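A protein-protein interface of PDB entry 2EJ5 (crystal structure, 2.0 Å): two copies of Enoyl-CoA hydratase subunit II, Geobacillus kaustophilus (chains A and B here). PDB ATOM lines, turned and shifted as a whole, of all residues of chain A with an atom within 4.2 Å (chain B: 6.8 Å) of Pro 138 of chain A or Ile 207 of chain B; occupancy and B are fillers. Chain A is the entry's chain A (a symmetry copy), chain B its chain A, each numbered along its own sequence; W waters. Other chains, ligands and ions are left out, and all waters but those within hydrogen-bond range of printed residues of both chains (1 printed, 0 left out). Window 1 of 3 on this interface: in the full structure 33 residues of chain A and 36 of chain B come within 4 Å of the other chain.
Of the 9 printed residues of chain A, 7 touch a printed residue of chain B. Of the 17 printed residues of chain B, 9 touch a printed residue of chain A. Among the printed residues, no Asp or Glu carboxylate lies within 4 Å of a Lys or Arg side-chain nitrogen of the other chain.
The side-chain amide nitrogen (NE2) of Gln 230 of chain B lies within hydrogen-bond range of the side-chain carboxylate (OD2) of Asp 139 of chain A (2.8 Å). NE2 of Gln 230 of chain B lies within hydrogen-bond range of O of Val 137 of chain A.
Printed residues of chain B within 4 Å of Pro 138 of chain A: Ile 207 (3.6 Å). Of the printed residues of chain B, His 142 of chain A touches Glu 226 (3.9 Å). Printed residues of chain A within 4 Å of Ile 207 of chain B: Val 137 (3.7 Å), Pro 138 (3.6 Å) and Val 160 (3.6 Å). Of the printed residues of chain A, Leu 211 of chain B touches Leu 156. Of the printed residues of chain A, Glu 226 of chain B touches Asp 139 and His 142. The nearest printed residue of chain B that does not touch Pro 138 of chain A is Glu 226 of chain B (4.2 Å). The nearest printed residue of chain A that does not touch Ile 207 of chain B is Leu 143 of chain A (4.04 Å). The nearest printed residue of chain A that does not touch Tyr 222 of chain B is Pro 138 of chain A (4.9 Å).
Among the printed residues, merely in contact across the chains: Val 137 of chain A with Ala 203 of chain B, Val 137 of chain A with Leu 206 of chain B, Val 137 of chain A with Ile 207 of chain B, Val 137 of chain A with Leu 210 of chain B, Pro 138 of chain A with Ile 207 of chain B, Asp 139 of chain A with Glu 226 of chain B, His 142 of chain A with Glu 226 of chain B, Leu 143 of chain A with Leu 210 of chain B, Leu 143 of chain A with Tyr 222 of chain B, Leu 156 of chain A with Leu 211 of chain B, Val 160 of chain A with Ile 204 of chain B and Val 160 of chain A with Ile 207 of chain B.
No position is printed for both chains. Of the 14 pairs that touch across the chains among the printed residues, none has its exchanged pair printed and touching as well.
Water W1 lies within hydrogen-bond range of the side-chain carboxylate of Glu 226 of chain B (2.6 Å), the side-chain hydroxyl of Tyr 222 of chain B (2.6 Å), the backbone carbonyl oxygen of Pro 138 of chain A (2.8 Å) and the backbone NH of Leu 143 of chain A (3.1 Å).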
ATOM      1  N   PHE A 131     -21.433  -5.259  -2.568  1.00  0.00           N
ATOM      2  CA  PHE A 131     -21.274  -4.131  -1.616  1.00  0.00           C
ATOM      3  C   PHE A 131     -19.970  -4.207  -0.784  1.00  0.00           C
ATOM      4  O   PHE A 131     -19.172  -3.239  -0.732  1.00  0.00           O
ATOM      5  CB  PHE A 131     -22.488  -4.090  -0.668  1.00  0.00           C
ATOM      6  CG  PHE A 131     -23.828  -4.165  -1.346  1.00  0.00           C
ATOM      7  CD1 PHE A 131     -24.488  -3.005  -1.738  1.00  0.00           C
ATOM      8  CD2 PHE A 131     -24.457  -5.418  -1.520  1.00  0.00           C
ATOM      9  CE1 PHE A 131     -25.771  -3.051  -2.300  1.00  0.00           C
ATOM     10  CE2 PHE A 131     -25.719  -5.498  -2.099  1.00  0.00           C
ATOM     11  CZ  PHE A 131     -26.393  -4.298  -2.489  1.00  0.00           C
ATOM     12  N   VAL A 137     -22.391  -1.834   2.943  1.00  0.00           N
ATOM     13  CA  VAL A 137     -23.287  -2.876   3.427  1.00  0.00           C
ATOM     14  C   VAL A 137     -24.344  -3.136   2.338  1.00  0.00           C
ATOM     15  O   VAL A 137     -24.652  -2.235   1.552  1.00  0.00           O
ATOM     16  CB  VAL A 137     -23.995  -2.465   4.767  1.00  0.00           C
ATOM     17  CG1 VAL A 137     -22.965  -2.084   5.860  1.00  0.00           C
ATOM     18  CG2 VAL A 137     -24.921  -1.310   4.555  1.00  0.00           C
ATOM     19  N   PRO A 138     -24.876  -4.377   2.259  1.00  0.00           N
ATOM     20  CA  PRO A 138     -25.990  -4.566   1.341  1.00  0.00           C
ATOM     21  C   PRO A 138     -27.166  -3.690   1.742  1.00  0.00           C
ATOM     22  O   PRO A 138     -27.495  -3.632   2.915  1.00  0.00           O
ATOM     23  CB  PRO A 138     -26.317  -6.061   1.476  1.00  0.00           C
ATOM     24  CG  PRO A 138     -24.940  -6.712   1.891  1.00  0.00           C
ATOM     25  CD  PRO A 138     -24.461  -5.644   2.902  1.00  0.00           C
ATOM     26  N   ASP A 139     -27.763  -3.015   0.767  1.00  0.00           N
ATOM     27  CA  ASP A 139     -28.814  -2.040   1.032  1.00  0.00           C
ATOM     28  C   ASP A 139     -30.041  -2.103   0.084  1.00  0.00           C
ATOM     29  O   ASP A 139     -30.194  -3.060  -0.664  1.00  0.00           O
ATOM     30  CB  ASP A 139     -28.209  -0.641   1.081  1.00  0.00           C
ATOM     31  CG  ASP A 139     -27.656  -0.186  -0.278  1.00  0.00           C
ATOM     32  OD1 ASP A 139     -27.930  -0.867  -1.315  1.00  0.00           O
ATOM     33  OD2 ASP A 139     -26.932   0.849  -0.300  1.00  0.00           O
ATOM     34  N   HIS A 142     -31.874  -5.275   1.205  1.00  0.00           N
ATOM     35  CA  HIS A 142     -31.207  -6.528   0.929  1.00  0.00           C
ATOM     36  C   HIS A 142     -31.264  -7.485   2.125  1.00  0.00           C
ATOM     37  O   HIS A 142     -31.688  -8.600   1.986  1.00  0.00           O
ATOM     38  CB  HIS A 142     -29.737  -6.268   0.600  1.00  0.00           C
ATOM     39  CG  HIS A 142     -29.094  -7.331  -0.228  1.00  0.00           C
ATOM     40  ND1 HIS A 142     -28.534  -8.471   0.310  1.00  0.00           N
ATOM     41  CD2 HIS A 142     -28.848  -7.386  -1.557  1.00  0.00           C
ATOM     42  CE1 HIS A 142     -28.010  -9.206  -0.653  1.00  0.00           C
ATOM     43  NE2 HIS A 142     -28.167  -8.558  -1.793  1.00  0.00           N
ATOM     44  N   LEU A 143     -30.821  -7.011   3.293  1.00  0.00           N
ATOM     45  CA  LEU A 143     -30.743  -7.833   4.480  1.00  0.00           C
ATOM     46  C   LEU A 143     -32.070  -8.029   5.213  1.00  0.00           C
ATOM     47  O   LEU A 143     -32.127  -8.744   6.207  1.00  0.00           O
ATOM     48  CB  LEU A 143     -29.640  -7.309   5.418  1.00  0.00           C
ATOM     49  CG  LEU A 143     -28.233  -7.326   4.795  1.00  0.00           C
ATOM     50  CD1 LEU A 143     -27.278  -6.638   5.793  1.00  0.00           C
ATOM     51  CD2 LEU A 143     -27.757  -8.700   4.451  1.00  0.00           C
ATOM     52  N   LEU A 156     -25.596 -14.046   5.773  1.00  0.00           N
ATOM     53  CA  LEU A 156     -24.337 -13.466   6.281  1.00  0.00           C
ATOM     54  C   LEU A 156     -23.145 -13.837   5.351  1.00  0.00           C
ATOM     55  O   LEU A 156     -22.320 -12.988   5.021  1.00  0.00           O
ATOM     56  CB  LEU A 156     -24.118 -13.881   7.740  1.00  0.00           C
ATOM     57  CG  LEU A 156     -22.970 -13.137   8.435  1.00  0.00           C
ATOM     58  CD1 LEU A 156     -23.242 -12.915   9.913  1.00  0.00           C
ATOM     59  CD2 LEU A 156     -21.700 -13.919   8.191  1.00  0.00           C
ATOM     60  N   ALA A 159     -23.507 -11.693   2.199  1.00  0.00           N
ATOM     61  CA  ALA A 159     -23.173 -10.313   2.519  1.00  0.00           C
ATOM     62  C   ALA A 159     -21.713 -10.103   2.877  1.00  0.00           C
ATOM     63  O   ALA A 159     -21.172  -9.035   2.590  1.00  0.00           O
ATOM     64  CB  ALA A 159     -24.053  -9.773   3.675  1.00  0.00           C
ATOM     65  N   VAL A 160     -21.091 -11.072   3.547  1.00  0.00           N
ATOM     66  CA  VAL A 160     -19.774 -10.840   4.139  1.00  0.00           C
ATOM     67  C   VAL A 160     -18.681 -11.254   3.191  1.00  0.00           C
ATOM     68  O   VAL A 160     -17.726 -10.495   2.963  1.00  0.00           O
ATOM     69  CB  VAL A 160     -19.606 -11.485   5.573  1.00  0.00           C
ATOM     70  CG1 VAL A 160     -18.128 -11.532   6.043  1.00  0.00           C
ATOM     71  CG2 VAL A 160     -20.477 -10.757   6.573  1.00  0.00           C
ATOM     72  N   GLU B  94     -19.573  -7.021  17.004  1.00  0.00           N
ATOM     73  CA  GLU B  94     -19.619  -6.575  15.606  1.00  0.00           C
ATOM     74  C   GLU B  94     -18.326  -6.889  14.834  1.00  0.00           C
ATOM     75  O   GLU B  94     -17.890  -6.086  13.994  1.00  0.00           O
ATOM     76  CB  GLU B  94     -19.760  -5.056  15.515  1.00  0.00           C
ATOM     77  CG  GLU B  94     -20.716  -4.320  16.434  1.00  0.00           C
ATOM     78  CD  GLU B  94     -22.107  -4.367  15.926  1.00  0.00           C
ATOM     79  OE1 GLU B  94     -22.368  -5.416  15.335  1.00  0.00           O
ATOM     80  OE2 GLU B  94     -22.935  -3.426  16.097  1.00  0.00           O
ATOM     81  N   LYS B 202     -15.377  -2.838   9.459  1.00  0.00           N
ATOM     82  CA  LYS B 202     -16.469  -1.928   9.901  1.00  0.00           C
ATOM     83  C   LYS B 202     -17.756  -2.197   9.121  1.00  0.00           C
ATOM     84  O   LYS B 202     -18.847  -2.106   9.664  1.00  0.00           O
ATOM     85  CB  LYS B 202     -16.109  -0.453   9.730  1.00  0.00           C
ATOM     86  CG  LYS B 202     -15.041   0.078  10.748  1.00  0.00           C
ATOM     87  CD  LYS B 202     -15.510   0.052  12.217  1.00  0.00           C
ATOM     88  CE  LYS B 202     -14.585   0.867  13.138  1.00  0.00           C
ATOM     89  NZ  LYS B 202     -13.256   1.046  12.559  1.00  0.00           N
ATOM     90  N   ALA B 203     -17.631  -2.485   7.830  1.00  0.00           N
ATOM     91  CA  ALA B 203     -18.812  -2.890   7.035  1.00  0.00           C
ATOM     92  C   ALA B 203     -19.354  -4.211   7.532  1.00  0.00           C
ATOM     93  O   ALA B 203     -20.565  -4.386   7.572  1.00  0.00           O
ATOM     94  CB  ALA B 203     -18.493  -2.966   5.560  1.00  0.00           C
ATOM     95  N   ILE B 204     -18.471  -5.123   7.924  1.00  0.00           N
ATOM     96  CA  ILE B 204     -18.920  -6.439   8.457  1.00  0.00           C
ATOM     97  C   ILE B 204     -19.682  -6.241   9.781  1.00  0.00           C
ATOM     98  O   ILE B 204     -20.696  -6.879  10.020  1.00  0.00           O
ATOM     99  CB  ILE B 204     -17.750  -7.431   8.652  1.00  0.00           C
ATOM    100  CG1 ILE B 204     -17.157  -7.826   7.268  1.00  0.00           C
ATOM    101  CG2 ILE B 204     -18.214  -8.709   9.422  1.00  0.00           C
ATOM    102  CD1 ILE B 204     -15.841  -8.608   7.401  1.00  0.00           C
ATOM    103  N   GLY B 205     -19.189  -5.362  10.645  1.00  0.00           N
ATOM    104  CA  GLY B 205     -19.920  -5.090  11.907  1.00  0.00           C
ATOM    105  C   GLY B 205     -21.299  -4.488  11.675  1.00  0.00           C
ATOM    106  O   GLY B 205     -22.285  -4.865  12.353  1.00  0.00           O
ATOM    107  N   LEU B 206     -21.389  -3.572  10.718  1.00  0.00           N
ATOM    108  CA  LEU B 206     -22.651  -2.935  10.345  1.00  0.00           C
ATOM    109  C   LEU B 206     -23.640  -3.921   9.694  1.00  0.00           C
ATOM    110  O   LEU B 206     -24.863  -3.837   9.881  1.00  0.00           O
ATOM    111  CB  LEU B 206     -22.352  -1.758   9.401  1.00  0.00           C
ATOM    112  CG  LEU B 206     -21.725  -0.499  10.084  1.00  0.00           C
ATOM    113  CD1 LEU B 206     -21.279   0.517   9.090  1.00  0.00           C
ATOM    114  CD2 LEU B 206     -22.610   0.142  11.141  1.00  0.00           C
ATOM    115  N   ILE B 207     -23.123  -4.864   8.916  1.00  0.00           N
ATOM    116  CA  ILE B 207     -24.039  -5.882   8.393  1.00  0.00           C
ATOM    117  C   ILE B 207     -24.568  -6.798   9.516  1.00  0.00           C
ATOM    118  O   ILE B 207     -25.776  -7.164   9.510  1.00  0.00           O
ATOM    119  CB  ILE B 207     -23.482  -6.670   7.174  1.00  0.00           C
ATOM    120  CG1 ILE B 207     -22.608  -7.818   7.611  1.00  0.00           C
ATOM    121  CG2 ILE B 207     -22.877  -5.763   6.118  1.00  0.00           C
ATOM    122  CD1 ILE B 207     -23.428  -9.097   7.673  1.00  0.00           C
ATOM    123  N   LYS B 208     -23.731  -7.141  10.488  1.00  0.00           N
ATOM    124  CA  LYS B 208     -24.230  -7.868  11.650  1.00  0.00           C
ATOM    125  C   LYS B 208     -25.270  -7.043  12.422  1.00  0.00           C
ATOM    126  O   LYS B 208     -26.254  -7.592  12.948  1.00  0.00           O
ATOM    127  CB  LYS B 208     -23.059  -8.244  12.552  1.00  0.00           C
ATOM    128  CG  LYS B 208     -22.271  -9.416  12.042  1.00  0.00           C
ATOM    129  CD  LYS B 208     -21.062  -9.716  12.908  1.00  0.00           C
ATOM    130  CE  LYS B 208     -21.486 -10.356  14.285  1.00  0.00           C
ATOM    131  NZ  LYS B 208     -20.478 -11.341  14.851  1.00  0.00           N
ATOM    132  N   ARG B 209     -25.041  -5.739  12.503  1.00  0.00           N
ATOM    133  CA  ARG B 209     -25.991  -4.839  13.171  1.00  0.00           C
ATOM    134  C   ARG B 209     -27.319  -4.884  12.419  1.00  0.00           C
ATOM    135  O   ARG B 209     -28.401  -5.033  13.035  1.00  0.00           O
ATOM    136  CB  ARG B 209     -25.446  -3.399  13.227  1.00  0.00           C
ATOM    137  CG  ARG B 209     -26.242  -2.455  14.136  1.00  0.00           C
ATOM    138  CD  ARG B 209     -25.628  -1.020  14.178  1.00  0.00           C
ATOM    139  NE  ARG B 209     -24.245  -1.013  14.679  1.00  0.00           N
ATOM    140  CZ  ARG B 209     -23.475   0.078  14.703  1.00  0.00           C
ATOM    141  NH1 ARG B 209     -23.950   1.233  14.264  1.00  0.00           N
ATOM    142  NH2 ARG B 209     -22.217   0.031  15.144  1.00  0.00           N
ATOM    143  N   LEU B 210     -27.243  -4.801  11.090  1.00  0.00           N
ATOM    144  CA  LEU B 210     -28.428  -4.824  10.269  1.00  0.00           C
ATOM    145  C   LEU B 210     -29.141  -6.166  10.282  1.00  0.00           C
ATOM    146  O   LEU B 210     -30.350  -6.209  10.137  1.00  0.00           O
ATOM    147  CB  LEU B 210     -28.109  -4.395   8.825  1.00  0.00           C
ATOM    148  CG  LEU B 210     -27.837  -2.906   8.588  1.00  0.00           C
ATOM    149  CD1 LEU B 210     -27.501  -2.697   7.108  1.00  0.00           C
ATOM    150  CD2 LEU B 210     -29.054  -2.067   8.988  1.00  0.00           C
ATOM    151  N   LEU B 211     -28.403  -7.271  10.385  1.00  0.00           N
ATOM    152  CA  LEU B 211     -29.045  -8.593  10.507  1.00  0.00           C
ATOM    153  C   LEU B 211     -29.844  -8.712  11.804  1.00  0.00           C
ATOM    154  O   LEU B 211     -30.888  -9.329  11.820  1.00  0.00           O
ATOM    155  CB  LEU B 211     -28.033  -9.747  10.385  1.00  0.00           C
ATOM    156  CG  LEU B 211     -27.542  -9.972   8.923  1.00  0.00           C
ATOM    157  CD1 LEU B 211     -26.384 -10.902   8.918  1.00  0.00           C
ATOM    158  CD2 LEU B 211     -28.684 -10.505   7.956  1.00  0.00           C
ATOM    159  N   ARG B 212     -29.341  -8.106  12.871  1.00  0.00           N
ATOM    160  CA  ARG B 212     -30.066  -7.954  14.136  1.00  0.00           C
ATOM    161  C   ARG B 212     -31.306  -7.101  13.928  1.00  0.00           C
ATOM    162  O   ARG B 212     -32.413  -7.524  14.323  1.00  0.00           O
ATOM    163  CB  ARG B 212     -29.168  -7.344  15.231  1.00  0.00           C
ATOM    164  CG  ARG B 212     -28.270  -8.380  15.917  1.00  0.00           C
ATOM    165  CD  ARG B 212     -27.023  -7.805  16.642  1.00  0.00           C
ATOM    166  NE  ARG B 212     -27.168  -6.490  17.276  1.00  0.00           N
ATOM    167  CZ  ARG B 212     -26.232  -5.535  17.270  1.00  0.00           C
ATOM    168  NH1 ARG B 212     -25.055  -5.704  16.646  1.00  0.00           N
ATOM    169  NH2 ARG B 212     -26.487  -4.382  17.888  1.00  0.00           N
ATOM    170  N   GLU B 213     -31.159  -5.947  13.271  1.00  0.00           N
ATOM    171  CA  GLU B 213     -32.325  -5.080  12.984  1.00  0.00           C
ATOM    172  C   GLU B 213     -33.388  -5.836  12.165  1.00  0.00           C
ATOM    173  O   GLU B 213     -34.595  -5.760  12.457  1.00  0.00           O
ATOM    174  CB  GLU B 213     -31.938  -3.804  12.231  1.00  0.00           C
ATOM    175  CG  GLU B 213     -31.108  -2.797  13.048  1.00  0.00           C
ATOM    176  CD  GLU B 213     -31.869  -2.106  14.196  1.00  0.00           C
ATOM    177  OE1 GLU B 213     -33.108  -2.213  14.310  1.00  0.00           O
ATOM    178  OE2 GLU B 213     -31.189  -1.427  14.973  1.00  0.00           O
ATOM    179  N   TYR B 222     -36.781  -0.755   9.266  1.00  0.00           N
ATOM    180  CA  TYR B 222     -35.549  -1.370   8.763  1.00  0.00           C
ATOM    181  C   TYR B 222     -34.803  -0.465   7.754  1.00  0.00           C
ATOM    182  O   TYR B 222     -33.594  -0.273   7.852  1.00  0.00           O
ATOM    183  CB  TYR B 222     -35.808  -2.742   8.124  1.00  0.00           C
ATOM    184  CG  TYR B 222     -34.502  -3.281   7.653  1.00  0.00           C
ATOM    185  CD1 TYR B 222     -33.627  -3.887   8.558  1.00  0.00           C
ATOM    186  CD2 TYR B 222     -34.091  -3.104   6.318  1.00  0.00           C
ATOM    187  CE1 TYR B 222     -32.368  -4.339   8.142  1.00  0.00           C
ATOM    188  CE2 TYR B 222     -32.825  -3.545   5.903  1.00  0.00           C
ATOM    189  CZ  TYR B 222     -31.985  -4.144   6.822  1.00  0.00           C
ATOM    190  OH  TYR B 222     -30.752  -4.558   6.448  1.00  0.00           O
ATOM    191  N   GLU B 226     -31.024   0.916   7.904  1.00  0.00           N
ATOM    192  CA  GLU B 226     -30.083   0.634   6.832  1.00  0.00           C
ATOM    193  C   GLU B 226     -29.370   1.886   6.321  1.00  0.00           C
ATOM    194  O   GLU B 226     -28.146   1.875   6.068  1.00  0.00           O
ATOM    195  CB  GLU B 226     -30.858  -0.011   5.696  1.00  0.00           C
ATOM    196  CG  GLU B 226     -30.026  -0.371   4.495  1.00  0.00           C
ATOM    197  CD  GLU B 226     -30.956  -0.774   3.334  1.00  0.00           C
ATOM    198  OE1 GLU B 226     -31.272   0.108   2.526  1.00  0.00           O
ATOM    199  OE2 GLU B 226     -31.371  -1.959   3.273  1.00  0.00           O
ATOM    200  N   CYS B 229     -26.712   3.019   8.678  1.00  0.00           N
ATOM    201  CA  CYS B 229     -25.507   2.162   8.582  1.00  0.00           C
ATOM    202  C   CYS B 229     -24.631   2.475   7.390  1.00  0.00           C
ATOM    203  O   CYS B 229     -23.402   2.422   7.494  1.00  0.00           O
ATOM    204  CB  CYS B 229     -25.886   0.686   8.572  1.00  0.00           C
ATOM    205  SG  CYS B 229     -26.467   0.203  10.180  1.00  0.00           S
ATOM    206  N   GLN B 230     -25.271   2.817   6.272  1.00  0.00           N
ATOM    207  CA  GLN B 230     -24.581   3.064   5.025  1.00  0.00           C
ATOM    208  C   GLN B 230     -23.928   4.437   5.040  1.00  0.00           C
ATOM    209  O   GLN B 230     -22.919   4.595   4.393  1.00  0.00           O
ATOM    210  CB  GLN B 230     -25.525   2.977   3.824  1.00  0.00           C
ATOM    211  CG  GLN B 230     -24.805   2.797   2.478  1.00  0.00           C
ATOM    212  CD  GLN B 230     -24.200   1.417   2.351  1.00  0.00           C
ATOM    213  OE1 GLN B 230     -23.296   1.011   3.136  1.00  0.00           O
ATOM    214  NE2 GLN B 230     -24.709   0.660   1.389  1.00  0.00           N
HETATM  215  O   HOH W   1     -30.003  -4.127   3.943  1.00  0.00           O
